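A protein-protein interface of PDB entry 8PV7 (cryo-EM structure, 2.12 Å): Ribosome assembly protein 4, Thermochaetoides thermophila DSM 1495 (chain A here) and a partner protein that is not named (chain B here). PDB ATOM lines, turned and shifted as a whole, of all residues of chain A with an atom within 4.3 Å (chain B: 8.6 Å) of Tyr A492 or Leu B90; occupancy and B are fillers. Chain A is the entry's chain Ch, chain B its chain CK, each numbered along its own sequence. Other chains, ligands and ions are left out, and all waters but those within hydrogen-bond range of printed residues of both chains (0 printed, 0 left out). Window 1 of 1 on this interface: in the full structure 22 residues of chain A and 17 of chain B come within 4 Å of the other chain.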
ATOM      1  N   PRO A 148     -35.048  32.327  14.953  1.00  0.00           N
ATOM      2  CA  PRO A 148     -34.335  31.613  13.883  1.00  0.00           C
ATOM      3  C   PRO A 148     -34.747  30.157  13.725  1.00  0.00           C
ATOM      4  O   PRO A 148     -35.062  29.463  14.691  1.00  0.00           O
ATOM      5  CB  PRO A 148     -32.871  31.721  14.315  1.00  0.00           C
ATOM      6  CG  PRO A 148     -32.804  32.997  14.994  1.00  0.00           C
ATOM      7  CD  PRO A 148     -34.106  33.173  15.714  1.00  0.00           C
ATOM      8  N   ILE A 149     -34.756  29.711  12.471  1.00  0.00           N
ATOM      9  CA  ILE A 149     -35.010  28.312  12.156  1.00  0.00           C
ATOM     10  C   ILE A 149     -33.770  27.493  12.475  1.00  0.00           C
ATOM     11  O   ILE A 149     -32.662  27.800  12.018  1.00  0.00           O
ATOM     12  CB  ILE A 149     -35.415  28.164  10.685  1.00  0.00           C
ATOM     13  CG1 ILE A 149     -36.635  29.033  10.397  1.00  0.00           C
ATOM     14  CG2 ILE A 149     -35.690  26.717  10.347  1.00  0.00           C
ATOM     15  CD1 ILE A 149     -36.959  29.144   8.956  1.00  0.00           C
ATOM     16  N   LEU A 150     -33.951  26.441  13.264  1.00  0.00           N
ATOM     17  CA  LEU A 150     -32.840  25.629  13.720  1.00  0.00           C
ATOM     18  C   LEU A 150     -32.814  24.242  13.106  1.00  0.00           C
ATOM     19  O   LEU A 150     -31.779  23.576  13.186  1.00  0.00           O
ATOM     20  CB  LEU A 150     -32.860  25.514  15.250  1.00  0.00           C
ATOM     21  CG  LEU A 150     -33.028  26.852  15.972  1.00  0.00           C
ATOM     22  CD1 LEU A 150     -33.159  26.656  17.468  1.00  0.00           C
ATOM     23  CD2 LEU A 150     -31.877  27.787  15.653  1.00  0.00           C
ATOM     24  N   TRP A 424     -15.297  24.982   8.381  1.00  0.00           N
ATOM     25  CA  TRP A 424     -15.232  26.341   8.889  1.00  0.00           C
ATOM     26  C   TRP A 424     -14.145  27.162   8.215  1.00  0.00           C
ATOM     27  O   TRP A 424     -13.933  28.314   8.595  1.00  0.00           O
ATOM     28  CB  TRP A 424     -14.999  26.333  10.398  1.00  0.00           C
ATOM     29  CG  TRP A 424     -16.184  25.932  11.207  1.00  0.00           C
ATOM     30  CD1 TRP A 424     -16.880  24.767  11.118  1.00  0.00           C
ATOM     31  CD2 TRP A 424     -16.808  26.693  12.239  1.00  0.00           C
ATOM     32  NE1 TRP A 424     -17.898  24.753  12.027  1.00  0.00           N
ATOM     33  CE2 TRP A 424     -17.880  25.927  12.729  1.00  0.00           C
ATOM     34  CE3 TRP A 424     -16.570  27.952  12.793  1.00  0.00           C
ATOM     35  CZ2 TRP A 424     -18.708  26.373  13.752  1.00  0.00           C
ATOM     36  CZ3 TRP A 424     -17.393  28.394  13.807  1.00  0.00           C
ATOM     37  CH2 TRP A 424     -18.450  27.605  14.276  1.00  0.00           C
ATOM     38  N   TYR A 450     -21.967  25.676   6.927  1.00  0.00           N
ATOM     39  CA  TYR A 450     -22.589  24.907   7.991  1.00  0.00           C
ATOM     40  C   TYR A 450     -23.193  23.603   7.510  1.00  0.00           C
ATOM     41  O   TYR A 450     -23.049  22.587   8.194  1.00  0.00           O
ATOM     42  CB  TYR A 450     -23.672  25.728   8.691  1.00  0.00           C
ATOM     43  CG  TYR A 450     -23.131  26.823   9.564  1.00  0.00           C
ATOM     44  CD1 TYR A 450     -21.936  26.666  10.247  1.00  0.00           C
ATOM     45  CD2 TYR A 450     -23.831  28.005   9.732  1.00  0.00           C
ATOM     46  CE1 TYR A 450     -21.448  27.665  11.056  1.00  0.00           C
ATOM     47  CE2 TYR A 450     -23.352  29.006  10.531  1.00  0.00           C
ATOM     48  CZ  TYR A 450     -22.162  28.833  11.193  1.00  0.00           C
ATOM     49  OH  TYR A 450     -21.688  29.834  11.997  1.00  0.00           O
ATOM     50  N   GLN A 451     -23.871  23.585   6.364  1.00  0.00           N
ATOM     51  CA  GLN A 451     -24.540  22.345   5.996  1.00  0.00           C
ATOM     52  C   GLN A 451     -24.340  22.043   4.522  1.00  0.00           C
ATOM     53  O   GLN A 451     -24.126  22.938   3.707  1.00  0.00           O
ATOM     54  CB  GLN A 451     -26.036  22.383   6.333  1.00  0.00           C
ATOM     55  CG  GLN A 451     -26.334  22.111   7.801  1.00  0.00           C
ATOM     56  CD  GLN A 451     -27.695  21.497   8.028  1.00  0.00           C
ATOM     57  OE1 GLN A 451     -28.331  21.000   7.103  1.00  0.00           O
ATOM     58  NE2 GLN A 451     -28.151  21.525   9.272  1.00  0.00           N
ATOM     59  N   GLU A 490     -27.655  34.410   8.612  1.00  0.00           N
ATOM     60  CA  GLU A 490     -26.945  33.141   8.466  1.00  0.00           C
ATOM     61  C   GLU A 490     -27.893  31.986   8.176  1.00  0.00           C
ATOM     62  O   GLU A 490     -29.031  31.960   8.646  1.00  0.00           O
ATOM     63  CB  GLU A 490     -26.148  32.829   9.734  1.00  0.00           C
ATOM     64  CG  GLU A 490     -25.264  33.949  10.223  1.00  0.00           C
ATOM     65  CD  GLU A 490     -24.484  33.566  11.463  1.00  0.00           C
ATOM     66  OE1 GLU A 490     -24.374  32.358  11.748  1.00  0.00           O
ATOM     67  OE2 GLU A 490     -23.984  34.474  12.155  1.00  0.00           O
ATOM     68  N   VAL A 491     -27.415  31.028   7.396  1.00  0.00           N
ATOM     69  CA  VAL A 491     -28.184  29.834   7.071  1.00  0.00           C
ATOM     70  C   VAL A 491     -27.797  28.724   8.038  1.00  0.00           C
ATOM     71  O   VAL A 491     -26.615  28.401   8.186  1.00  0.00           O
ATOM     72  CB  VAL A 491     -27.947  29.405   5.614  1.00  0.00           C
ATOM     73  CG1 VAL A 491     -28.669  28.110   5.323  1.00  0.00           C
ATOM     74  CG2 VAL A 491     -28.405  30.497   4.665  1.00  0.00           C
ATOM     75  N   TYR A 492     -28.795  28.143   8.698  1.00  0.00           N
ATOM     76  CA  TYR A 492     -28.577  27.075   9.661  1.00  0.00           C
ATOM     77  C   TYR A 492     -28.958  25.698   9.146  1.00  0.00           C
ATOM     78  O   TYR A 492     -28.221  24.744   9.380  1.00  0.00           O
ATOM     79  CB  TYR A 492     -29.360  27.352  10.950  1.00  0.00           C
ATOM     80  CG  TYR A 492     -28.798  28.482  11.772  1.00  0.00           C
ATOM     81  CD1 TYR A 492     -27.435  28.718  11.809  1.00  0.00           C
ATOM     82  CD2 TYR A 492     -29.628  29.311  12.514  1.00  0.00           C
ATOM     83  CE1 TYR A 492     -26.913  29.742  12.552  1.00  0.00           C
ATOM     84  CE2 TYR A 492     -29.115  30.339  13.264  1.00  0.00           C
ATOM     85  CZ  TYR A 492     -27.753  30.550  13.277  1.00  0.00           C
ATOM     86  OH  TYR A 492     -27.221  31.569  14.019  1.00  0.00           O
ATOM     87  N   ALA A 493     -30.083  25.572   8.450  1.00  0.00           N
ATOM     88  CA  ALA A 493     -30.623  24.286   8.045  1.00  0.00           C
ATOM     89  C   ALA A 493     -30.850  24.260   6.542  1.00  0.00           C
ATOM     90  O   ALA A 493     -31.420  25.192   5.973  1.00  0.00           O
ATOM     91  CB  ALA A 493     -31.931  23.991   8.775  1.00  0.00           C
ATOM     92  N   GLY A 506     -33.248  27.448   5.931  1.00  0.00           N
ATOM     93  CA  GLY A 506     -33.761  28.216   7.050  1.00  0.00           C
ATOM     94  C   GLY A 506     -32.621  28.664   7.927  1.00  0.00           C
ATOM     95  O   GLY A 506     -31.596  27.989   8.036  1.00  0.00           O
ATOM     96  N   GLY A 507     -32.792  29.819   8.546  1.00  0.00           N
ATOM     97  CA  GLY A 507     -31.735  30.319   9.390  1.00  0.00           C
ATOM     98  C   GLY A 507     -32.134  31.466  10.285  1.00  0.00           C
ATOM     99  O   GLY A 507     -33.243  31.504  10.812  1.00  0.00           O
ATOM    100  N   LYS A 508     -31.224  32.420  10.438  1.00  0.00           N
ATOM    101  CA  LYS A 508     -31.382  33.487  11.409  1.00  0.00           C
ATOM    102  C   LYS A 508     -32.370  34.563  10.970  1.00  0.00           C
ATOM    103  O   LYS A 508     -32.807  35.352  11.811  1.00  0.00           O
ATOM    104  CB  LYS A 508     -30.018  34.110  11.693  1.00  0.00           C
ATOM    105  CG  LYS A 508     -29.837  34.678  13.073  1.00  0.00           C
ATOM    106  CD  LYS A 508     -28.413  35.150  13.250  1.00  0.00           C
ATOM    107  CE  LYS A 508     -28.262  35.962  14.510  1.00  0.00           C
ATOM    108  NZ  LYS A 508     -26.911  36.563  14.608  1.00  0.00           N
ATOM    109  N   PRO B  82     -28.101  29.565  26.269  1.00  0.00           N
ATOM    110  CA  PRO B  82     -27.671  30.801  25.615  1.00  0.00           C
ATOM    111  C   PRO B  82     -28.824  31.782  25.427  1.00  0.00           C
ATOM    112  O   PRO B  82     -29.937  31.500  25.863  1.00  0.00           O
ATOM    113  CB  PRO B  82     -27.139  30.314  24.265  1.00  0.00           C
ATOM    114  CG  PRO B  82     -26.801  28.854  24.469  1.00  0.00           C
ATOM    115  CD  PRO B  82     -27.313  28.410  25.813  1.00  0.00           C
ATOM    116  N   ASP B  84     -29.449  33.923  22.173  1.00  0.00           N
ATOM    117  CA  ASP B  84     -30.010  33.795  20.836  1.00  0.00           C
ATOM    118  C   ASP B  84     -30.105  32.324  20.444  1.00  0.00           C
ATOM    119  O   ASP B  84     -29.165  31.562  20.677  1.00  0.00           O
ATOM    120  CB  ASP B  84     -29.158  34.545  19.820  1.00  0.00           C
ATOM    121  CG  ASP B  84     -28.940  35.991  20.203  1.00  0.00           C
ATOM    122  OD1 ASP B  84     -28.385  36.748  19.381  1.00  0.00           O
ATOM    123  OD2 ASP B  84     -29.324  36.371  21.328  1.00  0.00           O
ATOM    124  N   PRO B  85     -31.225  31.905  19.857  1.00  0.00           N
ATOM    125  CA  PRO B  85     -31.368  30.504  19.440  1.00  0.00           C
ATOM    126  C   PRO B  85     -30.374  30.122  18.352  1.00  0.00           C
ATOM    127  O   PRO B  85     -30.278  30.771  17.310  1.00  0.00           O
ATOM    128  CB  PRO B  85     -32.814  30.433  18.943  1.00  0.00           C
ATOM    129  CG  PRO B  85     -33.500  31.553  19.633  1.00  0.00           C
ATOM    130  CD  PRO B  85     -32.489  32.644  19.726  1.00  0.00           C
ATOM    131  N   ILE B  86     -29.625  29.058  18.617  1.00  0.00           N
ATOM    132  CA  ILE B  86     -28.597  28.553  17.711  1.00  0.00           C
ATOM    133  C   ILE B  86     -28.848  27.066  17.509  1.00  0.00           C
ATOM    134  O   ILE B  86     -29.550  26.433  18.310  1.00  0.00           O
ATOM    135  CB  ILE B  86     -27.174  28.816  18.259  1.00  0.00           C
ATOM    136  CG1 ILE B  86     -27.051  28.328  19.701  1.00  0.00           C
ATOM    137  CG2 ILE B  86     -26.803  30.275  18.117  1.00  0.00           C
ATOM    138  CD1 ILE B  86     -25.665  28.416  20.253  1.00  0.00           C
ATOM    139  N   PRO B  87     -28.317  26.480  16.438  1.00  0.00           N
ATOM    140  CA  PRO B  87     -28.451  25.032  16.271  1.00  0.00           C
ATOM    141  C   PRO B  87     -27.574  24.252  17.240  1.00  0.00           C
ATOM    142  O   PRO B  87     -26.747  24.799  17.979  1.00  0.00           O
ATOM    143  CB  PRO B  87     -28.016  24.788  14.822  1.00  0.00           C
ATOM    144  CG  PRO B  87     -27.998  26.085  14.186  1.00  0.00           C
ATOM    145  CD  PRO B  87     -27.762  27.106  15.225  1.00  0.00           C
ATOM    146  N   SER B  88     -27.781  22.934  17.219  1.00  0.00           N
ATOM    147  CA  SER B  88     -27.066  22.048  18.128  1.00  0.00           C
ATOM    148  C   SER B  88     -25.571  22.018  17.840  1.00  0.00           C
ATOM    149  O   SER B  88     -24.770  21.962  18.776  1.00  0.00           O
ATOM    150  CB  SER B  88     -27.667  20.644  18.067  1.00  0.00           C
ATOM    151  OG  SER B  88     -27.579  20.110  16.763  1.00  0.00           O
ATOM    152  N   TYR B  89     -25.170  22.080  16.566  1.00  0.00           N
ATOM    153  CA  TYR B  89     -23.747  22.094  16.253  1.00  0.00           C
ATOM    154  C   TYR B  89     -23.062  23.392  16.663  1.00  0.00           C
ATOM    155  O   TYR B  89     -21.838  23.405  16.797  1.00  0.00           O
ATOM    156  CB  TYR B  89     -23.510  21.818  14.760  1.00  0.00           C
ATOM    157  CG  TYR B  89     -24.236  22.715  13.783  1.00  0.00           C
ATOM    158  CD1 TYR B  89     -23.750  23.976  13.471  1.00  0.00           C
ATOM    159  CD2 TYR B  89     -25.383  22.279  13.138  1.00  0.00           C
ATOM    160  CE1 TYR B  89     -24.402  24.785  12.574  1.00  0.00           C
ATOM    161  CE2 TYR B  89     -26.041  23.078  12.238  1.00  0.00           C
ATOM    162  CZ  TYR B  89     -25.547  24.331  11.960  1.00  0.00           C
ATOM    163  OH  TYR B  89     -26.201  25.132  11.064  1.00  0.00           O
ATOM    164  N   LEU B  90     -23.809  24.470  16.873  1.00  0.00           N
ATOM    165  CA  LEU B  90     -23.250  25.700  17.410  1.00  0.00           C
ATOM    166  C   LEU B  90     -23.407  25.815  18.920  1.00  0.00           C
ATOM    167  O   LEU B  90     -22.820  26.723  19.513  1.00  0.00           O
ATOM    168  CB  LEU B  90     -23.884  26.918  16.731  1.00  0.00           C
ATOM    169  CG  LEU B  90     -23.513  27.133  15.264  1.00  0.00           C
ATOM    170  CD1 LEU B  90     -24.087  28.436  14.742  1.00  0.00           C
ATOM    171  CD2 LEU B  90     -22.011  27.091  15.068  1.00  0.00           C
ATOM    172  N   LEU B  91     -24.169  24.923  19.551  1.00  0.00           N
ATOM    173  CA  LEU B  91     -24.261  24.915  21.009  1.00  0.00           C
ATOM    174  C   LEU B  91     -22.914  24.605  21.659  1.00  0.00           C
ATOM    175  O   LEU B  91     -22.088  23.869  21.112  1.00  0.00           O
ATOM    176  CB  LEU B  91     -25.292  23.891  21.481  1.00  0.00           C
ATOM    177  CG  LEU B  91     -26.762  24.271  21.328  1.00  0.00           C
ATOM    178  CD1 LEU B  91     -27.649  23.107  21.693  1.00  0.00           C
ATOM    179  CD2 LEU B  91     -27.096  25.492  22.161  1.00  0.00           C
ATOM    180  N   ASP B  92     -22.700  25.204  22.832  1.00  0.00           N
ATOM    181  CA  ASP B  92     -21.537  25.080  23.714  1.00  0.00           C
ATOM    182  C   ASP B  92     -20.260  25.673  23.136  1.00  0.00           C
ATOM    183  O   ASP B  92     -19.191  25.468  23.716  1.00  0.00           O
ATOM    184  CB  ASP B  92     -21.243  23.628  24.121  1.00  0.00           C
ATOM    185  CG  ASP B  92     -22.131  23.149  25.232  1.00  0.00           C
ATOM    186  OD1 ASP B  92     -22.539  21.971  25.194  1.00  0.00           O
ATOM    187  OD2 ASP B  92     -22.433  23.945  26.142  1.00  0.00           O
ATOM    188  N   ARG B  93     -20.324  26.394  22.026  1.00  0.00           N
ATOM    189  CA  ARG B  93     -19.166  27.089  21.493  1.00  0.00           C
ATOM    190  C   ARG B  93     -19.117  28.504  22.050  1.00  0.00           C
ATOM    191  O   ARG B  93     -20.091  29.012  22.608  1.00  0.00           O
ATOM    192  CB  ARG B  93     -19.200  27.130  19.964  1.00  0.00           C
ATOM    193  CG  ARG B  93     -19.347  25.781  19.307  1.00  0.00           C
ATOM    194  CD  ARG B  93     -19.143  25.872  17.811  1.00  0.00           C
ATOM    195  NE  ARG B  93     -19.143  24.557  17.182  1.00  0.00           N
ATOM    196  CZ  ARG B  93     -18.106  23.732  17.169  1.00  0.00           C
ATOM    197  NH1 ARG B  93     -16.964  24.048  17.750  1.00  0.00           N
ATOM    198  NH2 ARG B  93     -18.221  22.558  16.561  1.00  0.00           N
ATOM    199  N   ALA B  94     -17.959  29.136  21.904  1.00  0.00           N
ATOM    200  CA  ALA B  94     -17.817  30.541  22.267  1.00  0.00           C
ATOM    201  C   ALA B  94     -18.411  31.398  21.158  1.00  0.00           C
ATOM    202  O   ALA B  94     -17.774  31.622  20.125  1.00  0.00           O
ATOM    203  CB  ALA B  94     -16.350  30.887  22.500  1.00  0.00           C
ATOM    204  N   ASN B  95     -19.635  31.873  21.365  1.00  0.00           N
ATOM    205  CA  ASN B  95     -20.331  32.685  20.389  1.00  0.00           C
ATOM    206  C   ASN B  95     -20.318  34.138  20.842  1.00  0.00           C
ATOM    207  O   ASN B  95     -20.314  34.400  22.054  1.00  0.00           O
ATOM    208  CB  ASN B  95     -21.778  32.201  20.213  1.00  0.00           C
ATOM    209  CG  ASN B  95     -21.865  30.715  19.908  1.00  0.00           C
ATOM    210  OD1 ASN B  95     -22.643  29.989  20.525  1.00  0.00           O
ATOM    211  ND2 ASN B  95     -21.075  30.260  18.945  1.00  0.00           N
ATOM    212  N   PRO B  96     -20.280  35.100  19.921  1.00  0.00           N
ATOM    213  CA  PRO B  96     -20.320  36.511  20.323  1.00  0.00           C
ATOM    214  C   PRO B  96     -21.654  36.874  20.963  1.00  0.00           C
ATOM    215  O   PRO B  96     -22.694  36.294  20.647  1.00  0.00           O
ATOM    216  CB  PRO B  96     -20.105  37.261  19.005  1.00  0.00           C
ATOM    217  CG  PRO B  96     -19.416  36.285  18.120  1.00  0.00           C
ATOM    218  CD  PRO B  96     -19.971  34.944  18.490  1.00  0.00           C
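Of the 14 printed residues of chain B, 6 touch a printed residue of chain A.
Hydrophobic or aromatic side chains of chain B within 4 Å of the printed part of chain A: Pro B87, Tyr B89 and Leu B90.
Printed residues of chain A that touch a printed residue of chain B: Leu A150, Trp A424, Tyr A450, Gln A451 and Tyr A492.
Among the printed residues, no Asp or Glu carboxylate lies within 4 Å of a Lys or Arg side-chain nitrogen of the other chain.
Pro B85 touches Leu A150.
Ile B86 touches Leu A150.
Leu A150 touches Pro B87.
Trp A424 touches Leu B90.
NE of Arg B93 touches CZ2 of Trp A424 (3.9 Å).
Tyr B89 touches Tyr A450 (OH to CB, 3.5 Å).
Leu B90 touches Tyr A450.
Tyr B89 touches Gln A451 (CE2 to NE2, 3.96 Å).
Tyr A492 touches Pro B87.
CD1 of Leu B90 touches CE1 of Tyr A492, 3.8 Å away.
NE of Arg B93 sits at hydrogen-bond distance from O of Tyr B89 (3.0 Å).
The backbone carbonyl oxygen of Leu B90 sits close to the side-chain amide oxygen of Asn B95 (3.4 Å).
The side-chain amide oxygen (OD1) of Asn B95 lies close to the backbone carbonyl oxygen (O) of Arg B93 (3.4 Å).
The side-chain amide nitrogen (NE2) of Gln A451 lies within hydrogen-bond range of the backbone carbonyl oxygen (O) of Tyr A492, 3.2 Å away.
N of Tyr A492 is in hydrogen-bond range of O of Gly A506, at 2.9 Å.
Of the printed residues of chain B, Tyr A450 touches Tyr B89 and Leu B90.
Of chain B, only Pro B87 (3.5 Å), Tyr B89 (2.7 Å) and Leu B90 (3.8 Å) come within 4 Å of Tyr A492.
Ala A493 touches none of the printed residues of chain B.
Of the printed residues of chain A, Pro B85 touches Leu A150 (3.8 Å).
Of chain A, only Trp A424, Tyr A450 and Tyr A492 come within 4 Å of Leu B90.
Ala B94 touches none of the printed residues of chain A.
The nearest residue of chain B that does not touch Tyr A492 is Pro B85 (4.2 Å).
The nearest printed residue of chain A that does not touch Leu B90 is Glu A490 (4.9 Å).
The side-chain hydroxyl (OH) of Tyr B89 lies within hydrogen-bond range of the backbone carbonyl oxygen (O) of Tyr A492, at 2.7 Å.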
